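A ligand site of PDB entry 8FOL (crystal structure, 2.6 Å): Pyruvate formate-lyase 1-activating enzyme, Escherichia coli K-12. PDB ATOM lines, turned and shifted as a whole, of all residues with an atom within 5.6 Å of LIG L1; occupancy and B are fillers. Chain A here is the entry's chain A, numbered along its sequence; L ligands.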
ATOM      1  N   CYS A  29      23.500  41.453 -14.015  1.00  0.00           N
ATOM      2  CA  CYS A  29      23.883  40.808 -12.767  1.00  0.00           C
ATOM      3  C   CYS A  29      25.266  41.296 -12.353  1.00  0.00           C
ATOM      4  O   CYS A  29      26.120  41.551 -13.210  1.00  0.00           O
ATOM      5  CB  CYS A  29      23.883  39.282 -12.898  1.00  0.00           C
ATOM      6  SG  CYS A  29      24.312  38.405 -11.371  1.00  0.00           S
ATOM      7  N   CYS A  33      29.526  34.123 -10.893  1.00  0.00           N
ATOM      8  CA  CYS A  33      29.610  32.702 -10.582  1.00  0.00           C
ATOM      9  C   CYS A  33      30.285  31.954 -11.724  1.00  0.00           C
ATOM     10  O   CYS A  33      29.897  32.074 -12.889  1.00  0.00           O
ATOM     11  CB  CYS A  33      28.225  32.117 -10.342  1.00  0.00           C
ATOM     12  SG  CYS A  33      27.189  33.046  -9.205  1.00  0.00           S
ATOM     13  N   TYR A  35      29.966  29.051 -12.541  1.00  0.00           N
ATOM     14  CA  TYR A  35      29.102  28.038 -13.129  1.00  0.00           C
ATOM     15  C   TYR A  35      27.884  28.622 -13.826  1.00  0.00           C
ATOM     16  O   TYR A  35      26.999  27.861 -14.228  1.00  0.00           O
ATOM     17  CB  TYR A  35      28.659  27.026 -12.051  1.00  0.00           C
ATOM     18  CG  TYR A  35      27.984  27.616 -10.829  1.00  0.00           C
ATOM     19  CD1 TYR A  35      26.700  28.152 -10.901  1.00  0.00           C
ATOM     20  CD2 TYR A  35      28.608  27.597  -9.583  1.00  0.00           C
ATOM     21  CE1 TYR A  35      26.078  28.674  -9.788  1.00  0.00           C
ATOM     22  CE2 TYR A  35      27.984  28.127  -8.459  1.00  0.00           C
ATOM     23  CZ  TYR A  35      26.713  28.663  -8.575  1.00  0.00           C
ATOM     24  OH  TYR A  35      26.076  29.188  -7.478  1.00  0.00           O
ATOM     25  N   CYS A  36      27.825  29.939 -14.012  1.00  0.00           N
ATOM     26  CA  CYS A  36      26.630  30.603 -14.527  1.00  0.00           C
ATOM     27  C   CYS A  36      26.208  30.023 -15.871  1.00  0.00           C
ATOM     28  O   CYS A  36      26.964  30.063 -16.841  1.00  0.00           O
ATOM     29  CB  CYS A  36      26.870  32.097 -14.664  1.00  0.00           C
ATOM     30  SG  CYS A  36      25.405  33.035 -15.145  1.00  0.00           S
ATOM     31  N   HIS A  37      24.989  29.498 -15.929  1.00  0.00           N
ATOM     32  CA  HIS A  37      24.465  28.986 -17.187  1.00  0.00           C
ATOM     33  C   HIS A  37      23.747  30.051 -18.002  1.00  0.00           C
ATOM     34  O   HIS A  37      23.267  29.767 -19.104  1.00  0.00           O
ATOM     35  CB  HIS A  37      23.530  27.787 -16.935  1.00  0.00           C
ATOM     36  CG  HIS A  37      22.315  28.091 -16.105  1.00  0.00           C
ATOM     37  ND1 HIS A  37      21.627  27.105 -15.420  1.00  0.00           N
ATOM     38  CD2 HIS A  37      21.660  29.250 -15.858  1.00  0.00           C
ATOM     39  CE1 HIS A  37      20.605  27.655 -14.788  1.00  0.00           C
ATOM     40  NE2 HIS A  37      20.599  28.947 -15.044  1.00  0.00           N
ATOM     41  N   ASN A  38      23.665  31.287 -17.487  1.00  0.00           N
ATOM     42  CA  ASN A  38      23.095  32.409 -18.233  1.00  0.00           C
ATOM     43  C   ASN A  38      24.117  33.528 -18.327  1.00  0.00           C
ATOM     44  O   ASN A  38      23.845  34.665 -17.932  1.00  0.00           O
ATOM     45  CB  ASN A  38      21.807  32.909 -17.562  1.00  0.00           C
ATOM     46  CG  ASN A  38      20.692  31.888 -17.602  1.00  0.00           C
ATOM     47  OD1 ASN A  38      20.637  31.040 -18.496  1.00  0.00           O
ATOM     48  ND2 ASN A  38      19.791  31.969 -16.638  1.00  0.00           N
ATOM     49  N   SER A  76      13.292  36.435 -12.842  1.00  0.00           N
ATOM     50  CA  SER A  76      14.578  35.753 -12.777  1.00  0.00           C
ATOM     51  C   SER A  76      15.616  36.498 -13.617  1.00  0.00           C
ATOM     52  O   SER A  76      15.500  37.712 -13.832  1.00  0.00           O
ATOM     53  CB  SER A  76      14.437  34.305 -13.246  1.00  0.00           C
ATOM     54  OG  SER A  76      15.653  33.587 -13.089  1.00  0.00           O
ATOM     55  N   GLY A  77      16.645  35.791 -14.093  1.00  0.00           N
ATOM     56  CA  GLY A  77      17.669  36.427 -14.890  1.00  0.00           C
ATOM     57  C   GLY A  77      18.972  35.655 -14.923  1.00  0.00           C
ATOM     58  O   GLY A  77      18.962  34.439 -15.163  1.00  0.00           O
ATOM     59  N   GLY A  78      20.092  36.318 -14.684  1.00  0.00           N
ATOM     60  CA  GLY A  78      20.113  37.718 -14.316  1.00  0.00           C
ATOM     61  C   GLY A  78      19.707  37.899 -12.866  1.00  0.00           C
ATOM     62  O   GLY A  78      19.295  36.951 -12.207  1.00  0.00           O
ATOM     63  N   GLU A  79      19.814  39.129 -12.359  1.00  0.00           N
ATOM     64  CA  GLU A  79      19.406  39.436 -11.000  1.00  0.00           C
ATOM     65  C   GLU A  79      18.265  40.446 -11.050  1.00  0.00           C
ATOM     66  O   GLU A  79      18.489  41.638 -11.290  1.00  0.00           O
ATOM     67  CB  GLU A  79      20.579  39.949 -10.172  1.00  0.00           C
ATOM     68  CG  GLU A  79      20.205  40.174  -8.725  1.00  0.00           C
ATOM     69  CD  GLU A  79      19.313  39.078  -8.173  1.00  0.00           C
ATOM     70  OE1 GLU A  79      19.676  37.884  -8.297  1.00  0.00           O
ATOM     71  OE2 GLU A  79      18.232  39.398  -7.639  1.00  0.00           O
ATOM     72  N   ASP A 104      13.275  35.118  -8.035  1.00  0.00           N
ATOM     73  CA  ASP A 104      14.452  34.266  -8.113  1.00  0.00           C
ATOM     74  C   ASP A 104      15.672  35.175  -8.007  1.00  0.00           C
ATOM     75  O   ASP A 104      16.067  35.815  -8.983  1.00  0.00           O
ATOM     76  CB  ASP A 104      14.442  33.457  -9.410  1.00  0.00           C
ATOM     77  CG  ASP A 104      15.407  32.288  -9.387  1.00  0.00           C
ATOM     78  OD1 ASP A 104      15.448  31.557  -8.372  1.00  0.00           O
ATOM     79  OD2 ASP A 104      16.119  32.088 -10.396  1.00  0.00           O
ATOM     80  N   THR A 105      16.255  35.251  -6.815  1.00  0.00           N
ATOM     81  CA  THR A 105      17.249  36.269  -6.496  1.00  0.00           C
ATOM     82  C   THR A 105      18.470  35.676  -5.809  1.00  0.00           C
ATOM     83  O   THR A 105      18.362  34.725  -5.029  1.00  0.00           O
ATOM     84  CB  THR A 105      16.688  37.360  -5.587  1.00  0.00           C
ATOM     85  OG1 THR A 105      17.718  38.295  -5.263  1.00  0.00           O
ATOM     86  CG2 THR A 105      16.163  36.754  -4.291  1.00  0.00           C
ATOM     87  N   ASN A 106      19.634  36.273  -6.073  1.00  0.00           N
ATOM     88  CA  ASN A 106      20.844  35.939  -5.348  1.00  0.00           C
ATOM     89  C   ASN A 106      21.010  36.739  -4.064  1.00  0.00           C
ATOM     90  O   ASN A 106      22.003  36.557  -3.350  1.00  0.00           O
ATOM     91  CB  ASN A 106      22.084  36.137  -6.237  1.00  0.00           C
ATOM     92  CG  ASN A 106      22.233  37.564  -6.727  1.00  0.00           C
ATOM     93  OD1 ASN A 106      21.671  38.501  -6.169  1.00  0.00           O
ATOM     94  ND2 ASN A 106      23.006  37.737  -7.799  1.00  0.00           N
ATOM     95  N   MET A 127      12.840  32.611  -3.928  1.00  0.00           N
ATOM     96  CA  MET A 127      13.811  31.539  -4.110  1.00  0.00           C
ATOM     97  C   MET A 127      15.198  32.173  -3.984  1.00  0.00           C
ATOM     98  O   MET A 127      15.676  32.828  -4.906  1.00  0.00           O
ATOM     99  CB  MET A 127      13.611  30.848  -5.459  1.00  0.00           C
ATOM    100  CG  MET A 127      12.225  30.232  -5.601  1.00  0.00           C
ATOM    101  SD  MET A 127      12.068  29.169  -7.054  1.00  0.00           S
ATOM    102  CE  MET A 127      12.518  30.325  -8.360  1.00  0.00           C
ATOM    103  N   ASP A 129      19.265  32.144  -3.386  1.00  0.00           N
ATOM    104  CA  ASP A 129      20.472  31.350  -3.613  1.00  0.00           C
ATOM    105  C   ASP A 129      21.495  31.659  -2.538  1.00  0.00           C
ATOM    106  O   ASP A 129      21.982  32.792  -2.447  1.00  0.00           O
ATOM    107  CB  ASP A 129      21.051  31.632  -4.996  1.00  0.00           C
ATOM    108  CG  ASP A 129      20.780  30.512  -5.970  1.00  0.00           C
ATOM    109  OD1 ASP A 129      19.591  30.178  -6.167  1.00  0.00           O
ATOM    110  OD2 ASP A 129      21.757  29.958  -6.534  1.00  0.00           O
ATOM    111  N   LYS A 131      24.974  30.505  -2.177  1.00  0.00           N
ATOM    112  CA  LYS A 131      25.906  29.797  -3.036  1.00  0.00           C
ATOM    113  C   LYS A 131      27.048  29.137  -2.263  1.00  0.00           C
ATOM    114  O   LYS A 131      27.552  28.093  -2.693  1.00  0.00           O
ATOM    115  CB  LYS A 131      26.457  30.753  -4.098  1.00  0.00           C
ATOM    116  CG  LYS A 131      25.371  31.238  -5.048  1.00  0.00           C
ATOM    117  CD  LYS A 131      25.843  32.369  -5.929  1.00  0.00           C
ATOM    118  CE  LYS A 131      24.682  32.952  -6.725  1.00  0.00           C
ATOM    119  NZ  LYS A 131      24.181  31.991  -7.739  1.00  0.00           N
ATOM    120  N   ARG A 166      18.040  27.753  -2.212  1.00  0.00           N
ATOM    121  CA  ARG A 166      18.616  27.012  -3.327  1.00  0.00           C
ATOM    122  C   ARG A 166      20.120  26.901  -3.134  1.00  0.00           C
ATOM    123  O   ARG A 166      20.808  27.919  -2.953  1.00  0.00           O
ATOM    124  CB  ARG A 166      18.296  27.681  -4.657  1.00  0.00           C
ATOM    125  CG  ARG A 166      16.837  27.594  -5.103  1.00  0.00           C
ATOM    126  CD  ARG A 166      16.556  26.270  -5.789  1.00  0.00           C
ATOM    127  NE  ARG A 166      15.182  26.151  -6.273  1.00  0.00           N
ATOM    128  CZ  ARG A 166      14.772  26.590  -7.463  1.00  0.00           C
ATOM    129  NH1 ARG A 166      15.626  27.184  -8.282  1.00  0.00           N
ATOM    130  NH2 ARG A 166      13.509  26.437  -7.817  1.00  0.00           N
ATOM    131  N   VAL A 168      23.401  25.238  -5.002  1.00  0.00           N
ATOM    132  CA  VAL A 168      23.984  24.575  -6.163  1.00  0.00           C
ATOM    133  C   VAL A 168      25.217  23.793  -5.709  1.00  0.00           C
ATOM    134  O   VAL A 168      26.208  24.376  -5.288  1.00  0.00           O
ATOM    135  CB  VAL A 168      24.332  25.578  -7.264  1.00  0.00           C
ATOM    136  CG1 VAL A 168      25.132  24.893  -8.375  1.00  0.00           C
ATOM    137  CG2 VAL A 168      23.072  26.201  -7.824  1.00  0.00           C
ATOM    138  N   LEU A 199      20.487  21.863  -5.846  1.00  0.00           N
ATOM    139  CA  LEU A 199      20.571  21.803  -7.295  1.00  0.00           C
ATOM    140  C   LEU A 199      21.914  21.219  -7.671  1.00  0.00           C
ATOM    141  O   LEU A 199      22.955  21.801  -7.343  1.00  0.00           O
ATOM    142  CB  LEU A 199      20.410  23.190  -7.908  1.00  0.00           C
ATOM    143  CG  LEU A 199      19.067  23.898  -7.707  1.00  0.00           C
ATOM    144  CD1 LEU A 199      19.114  25.298  -8.311  1.00  0.00           C
ATOM    145  CD2 LEU A 199      17.931  23.084  -8.312  1.00  0.00           C
ATOM    146  N   PRO A 200      21.950  20.065  -8.345  1.00  0.00           N
ATOM    147  CA  PRO A 200      23.229  19.542  -8.836  1.00  0.00           C
ATOM    148  C   PRO A 200      23.805  20.427  -9.935  1.00  0.00           C
ATOM    149  O   PRO A 200      23.069  20.995 -10.743  1.00  0.00           O
ATOM    150  CB  PRO A 200      22.852  18.155  -9.367  1.00  0.00           C
ATOM    151  CG  PRO A 200      21.387  18.251  -9.688  1.00  0.00           C
ATOM    152  CD  PRO A 200      20.814  19.185  -8.656  1.00  0.00           C
ATOM    153  N   TYR A 201      25.131  20.545  -9.926  1.00  0.00           N
ATOM    154  CA  TYR A 201      25.811  21.318 -10.961  1.00  0.00           C
ATOM    155  C   TYR A 201      25.675  20.643 -12.318  1.00  0.00           C
ATOM    156  O   TYR A 201      25.799  19.422 -12.437  1.00  0.00           O
ATOM    157  CB  TYR A 201      27.288  21.496 -10.608  1.00  0.00           C
ATOM    158  CG  TYR A 201      28.145  21.913 -11.786  1.00  0.00           C
ATOM    159  CD1 TYR A 201      28.161  23.221 -12.223  1.00  0.00           C
ATOM    160  CD2 TYR A 201      28.926  20.979 -12.466  1.00  0.00           C
ATOM    161  CE1 TYR A 201      28.936  23.608 -13.308  1.00  0.00           C
ATOM    162  CE2 TYR A 201      29.696  21.358 -13.555  1.00  0.00           C
ATOM    163  CZ  TYR A 201      29.691  22.669 -13.971  1.00  0.00           C
ATOM    164  OH  TYR A 201      30.464  23.051 -15.043  1.00  0.00           O
ATOM    165  N   HIS A 202      25.425  21.452 -13.354  1.00  0.00           N
ATOM    166  CA  HIS A 202      25.386  20.988 -14.729  1.00  0.00           C
ATOM    167  C   HIS A 202      26.185  21.935 -15.610  1.00  0.00           C
ATOM    168  O   HIS A 202      26.315  23.127 -15.302  1.00  0.00           O
ATOM    169  CB  HIS A 202      23.939  20.875 -15.274  1.00  0.00           C
ATOM    170  CG  HIS A 202      23.135  22.134 -15.176  1.00  0.00           C
ATOM    171  ND1 HIS A 202      21.976  22.223 -14.431  1.00  0.00           N
ATOM    172  CD2 HIS A 202      23.316  23.358 -15.720  1.00  0.00           C
ATOM    173  CE1 HIS A 202      21.482  23.440 -14.528  1.00  0.00           C
ATOM    174  NE2 HIS A 202      22.284  24.155 -15.303  1.00  0.00           N
ATOM    175  N   GLU A 203      26.728  21.399 -16.701  1.00  0.00           N
ATOM    176  CA  GLU A 203      27.568  22.172 -17.602  1.00  0.00           C
ATOM    177  C   GLU A 203      26.767  22.901 -18.669  1.00  0.00           C
ATOM    178  O   GLU A 203      27.360  23.428 -19.615  1.00  0.00           O
ATOM    179  CB  GLU A 203      28.605  21.247 -18.268  1.00  0.00           C
ATOM    180  CG  GLU A 203      29.907  21.947 -18.636  1.00  0.00           C
ATOM    181  CD  GLU A 203      30.844  21.063 -19.437  1.00  0.00           C
ATOM    182  OE1 GLU A 203      30.372  20.097 -20.079  1.00  0.00           O
ATOM    183  OE2 GLU A 203      32.068  21.334 -19.424  1.00  0.00           O
ATOM    184  N   LEU A 204      25.436  22.939 -18.548  1.00  0.00           N
ATOM    185  CA  LEU A 204      24.617  23.641 -19.529  1.00  0.00           C
ATOM    186  C   LEU A 204      24.972  25.124 -19.535  1.00  0.00           C
ATOM    187  O   LEU A 204      25.248  25.723 -18.497  1.00  0.00           O
ATOM    188  CB  LEU A 204      23.134  23.448 -19.215  1.00  0.00           C
ATOM    189  CG  LEU A 204      22.622  22.014 -19.061  1.00  0.00           C
ATOM    190  CD1 LEU A 204      21.116  22.010 -18.811  1.00  0.00           C
ATOM    191  CD2 LEU A 204      22.967  21.154 -20.278  1.00  0.00           C
ATOM    192  N   TYR A 216      35.629  29.142 -19.858  1.00  0.00           N
ATOM    193  CA  TYR A 216      34.819  28.544 -18.807  1.00  0.00           C
ATOM    194  C   TYR A 216      35.744  27.899 -17.784  1.00  0.00           C
ATOM    195  O   TYR A 216      36.485  26.968 -18.105  1.00  0.00           O
ATOM    196  CB  TYR A 216      33.854  27.523 -19.412  1.00  0.00           C
ATOM    197  CG  TYR A 216      32.820  26.982 -18.453  1.00  0.00           C
ATOM    198  CD1 TYR A 216      31.846  27.813 -17.910  1.00  0.00           C
ATOM    199  CD2 TYR A 216      32.799  25.633 -18.114  1.00  0.00           C
ATOM    200  CE1 TYR A 216      30.892  27.312 -17.032  1.00  0.00           C
ATOM    201  CE2 TYR A 216      31.852  25.130 -17.244  1.00  0.00           C
ATOM    202  CZ  TYR A 216      30.895  25.977 -16.701  1.00  0.00           C
ATOM    203  OH  TYR A 216      29.950  25.465 -15.841  1.00  0.00           O
HETATM  204  N1  LIG L   1      20.697  35.276 -10.644  1.00  0.00           N
HETATM  205  C1  LIG L   1      19.822  34.586  -9.718  1.00  0.00           C
HETATM  206  C2  LIG L   1      20.630  33.569  -8.904  1.00  0.00           C
HETATM  207  O1  LIG L   1      21.638  33.007  -9.406  1.00  0.00           O
HETATM  208  O2  LIG L   1      20.283  33.295  -7.730  1.00  0.00           O
HETATM  209  C3  LIG L   1      18.682  33.886 -10.472  1.00  0.00           C
HETATM  210  C4  LIG L   1      19.105  33.511 -11.891  1.00  0.00           C
HETATM  211  S1  LIG L   1      19.877  31.960 -11.924  1.00  0.00           S
HETATM  212  C5  LIG L   1      20.813  31.823 -13.373  1.00  0.00           C
HETATM  213  C6  LIG L   1      18.706  30.711 -11.819  1.00  0.00           C
HETATM  214  C7  LIG L   1      19.192  29.443 -11.023  1.00  0.00           C
HETATM  215  O3  LIG L   1      20.077  28.582 -11.837  1.00  0.00           O
HETATM  216  C8  LIG L   1      19.984  29.793  -9.743  1.00  0.00           C
HETATM  217  O4  LIG L   1      19.572  28.943  -8.656  1.00  0.00           O
HETATM  218  C9  LIG L   1      21.415  29.467 -10.152  1.00  0.00           C
HETATM  219  O5  LIG L   1      22.244  29.210  -8.994  1.00  0.00           O
HETATM  220  C10 LIG L   1      21.180  28.184 -10.967  1.00  0.00           C
HETATM  221  N2  LIG L   1      22.340  27.848 -11.763  1.00  0.00           N
HETATM  222  C11 LIG L   1      23.122  28.695 -12.448  1.00  0.00           C
HETATM  223  N3  LIG L   1      24.084  27.967 -13.046  1.00  0.00           N
HETATM  224  C12 LIG L   1      23.897  26.685 -12.728  1.00  0.00           C
HETATM  225  C13 LIG L   1      24.590  25.531 -13.067  1.00  0.00           C
HETATM  226  N4  LIG L   1      25.753  25.614 -13.931  1.00  0.00           N
HETATM  227  N5  LIG L   1      24.186  24.367 -12.598  1.00  0.00           N
HETATM  228  C14 LIG L   1      23.102  24.290 -11.797  1.00  0.00           C
HETATM  229  N6  LIG L   1      22.425  25.414 -11.466  1.00  0.00           N
HETATM  230  C15 LIG L   1      22.820  26.607 -11.934  1.00  0.00           C
HETATM  231 FE1  LG2 L   2      25.551  33.882 -10.532  1.00  0.00          FE
HETATM  232 FE2  LG2 L   2      22.874  33.896 -11.152  1.00  0.00          FE
HETATM  233 FE3  LG2 L   2      24.755  33.892 -13.151  1.00  0.00          FE
HETATM  234 FE4  LG2 L   2      24.402  36.131 -11.592  1.00  0.00          FE
HETATM  235  S1  LG2 L   2      22.891  35.213 -13.032  1.00  0.00           S
HETATM  236  S2  LG2 L   2      26.389  35.174 -12.208  1.00  0.00           S
HETATM  237  S3  LG2 L   2      23.927  35.176  -9.582  1.00  0.00           S
HETATM  238  S4  LG2 L   2      24.380  32.251 -11.616  1.00  0.00           S
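The side-chain amino group (NZ) of Lys 131 sits close to an oxygen (O1) of LIG L1 (3.2 Å).
An iron atom (FE3) of LG2 L2 is bound by the side-chain sulfur of Cys 36 (2.3 Å).
O of Tyr 35 sits at hydrogen-bond distance from N4 of LIG L1, 2.6 Å away.
A nitrogen (N5) of LIG L1 lies within hydrogen-bond range of a ring nitrogen (NE2) of His 202 (3.3 Å).
An oxygen (O5) of LIG L1 sits at hydrogen-bond distance from the side-chain carboxylate (OD2) of Asp 129 (2.6 Å).
OE1 of Glu 79 is in salt-bridge range of N1 of LIG L1, 3.7 Å away.
A nitrogen (N3) of LIG L1 lies within hydrogen-bond range of the backbone NH of His 37, at 3.4 Å.
N1 of LIG L1 lies within hydrogen-bond range of O of Gly 78 (2.7 Å).
N of Asn 106 lies within hydrogen-bond range of O2 of LIG L1.
The backbone NH of Gly 78 lies close to a sulfur (S1) of LG2 L2.
The side-chain sulfur of Cys 33 binds an iron atom (FE1) of LG2 L2, 2.3 Å away.
NZ of Lys 131 lies close to S3 of LG2 L2 (3.7 Å).
The backbone carbonyl oxygen (O) of His 202 is in hydrogen-bond range of a nitrogen (N4) of LIG L1, 2.9 Å away.
NE2 of His 37 sits close to O3 of LIG L1 (3.3 Å).
The backbone NH of Cys 33 sits close to a sulfur (S2) of LG2 L2 (3.6 Å).
The side-chain amide nitrogen of Asn 106 lies close to a sulfur (S3) of LG2 L2 (3.3 Å).
FE4 of LG2 L2 is bound by SG of Cys 29.
A nitrogen (N5) of LIG L1 is in hydrogen-bond range of the backbone NH of His 202 (3.3 Å).
Cys 36 touches LIG L1.
ND2 of Asn 38 touches C5 of LIG L1, 3.4 Å away.
Ser 76 touches LIG L1.
Gly 77 touches LIG L1 (O to C4, 3.4 Å).
OD2 of Asp 104 touches C3 of LIG L1 (3.1 Å).
Thr 105 touches LIG L1 (C to O2, 3.6 Å).
Val 168 touches LIG L1.
Leu 199 touches LIG L1.
O of Pro 200 touches C14 of LIG L1, at 3.5 Å.
Tyr 201 touches LIG L1 (CD1 to N4, 3.8 Å).
Hydrophobic or aromatic side chains that line LIG L1: Tyr 35, His 37, Val 168, Leu 199, Tyr 201 and His 202.
Within 4 Å of LIG L1: Tyr 35, Cys 36, His 37, Asn 38, Ser 76, Gly 77, Gly 78, Glu 79, Asp 104, Thr 105, Asn 106, Asp 129, Lys 131, Val 168, Leu 199, Pro 200, Tyr 201 and His 202.
Along chain A the residues within 4 Å of LIG L1 span positions 35 to 202.
The nearest printed residue that does not touch LIG L1 is Arg 166 (4.3 Å).
The backbone NH (N) of Asn 106 sits at hydrogen-bond distance from the side-chain carboxylate (OE1) of Glu 79, 2.7 Å away.
The backbone carbonyl oxygen (O) of Gly 77 lies within hydrogen-bond range of the side-chain amide nitrogen (ND2) of Asn 38 (3.0 Å).
The backbone carbonyl oxygen (O) of Thr 105 is in hydrogen-bond range of the backbone NH (N) of Asp 129.
The side-chain sulfur (SG) of Cys 33 sits close to the side-chain amino group (NZ) of Lys 131, 3.5 Å away.
The side-chain amino group (NZ) of Lys 131 lies close to the side-chain hydroxyl (OH) of Tyr 35 (3.4 Å).
OH of Tyr 201 is in hydrogen-bond range of OH of Tyr 216 (2.6 Å).
The backbone NH of Asn 38 sits close to the side-chain sulfur of Cys 36 (3.4 Å).
NE2 of His 202 is in hydrogen-bond range of ND1 of His 37 (3.0 Å).
An oxygen (O1) of LIG L1 is bound to an iron atom (FE2) of LG2 L2, 2.3 Å away.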
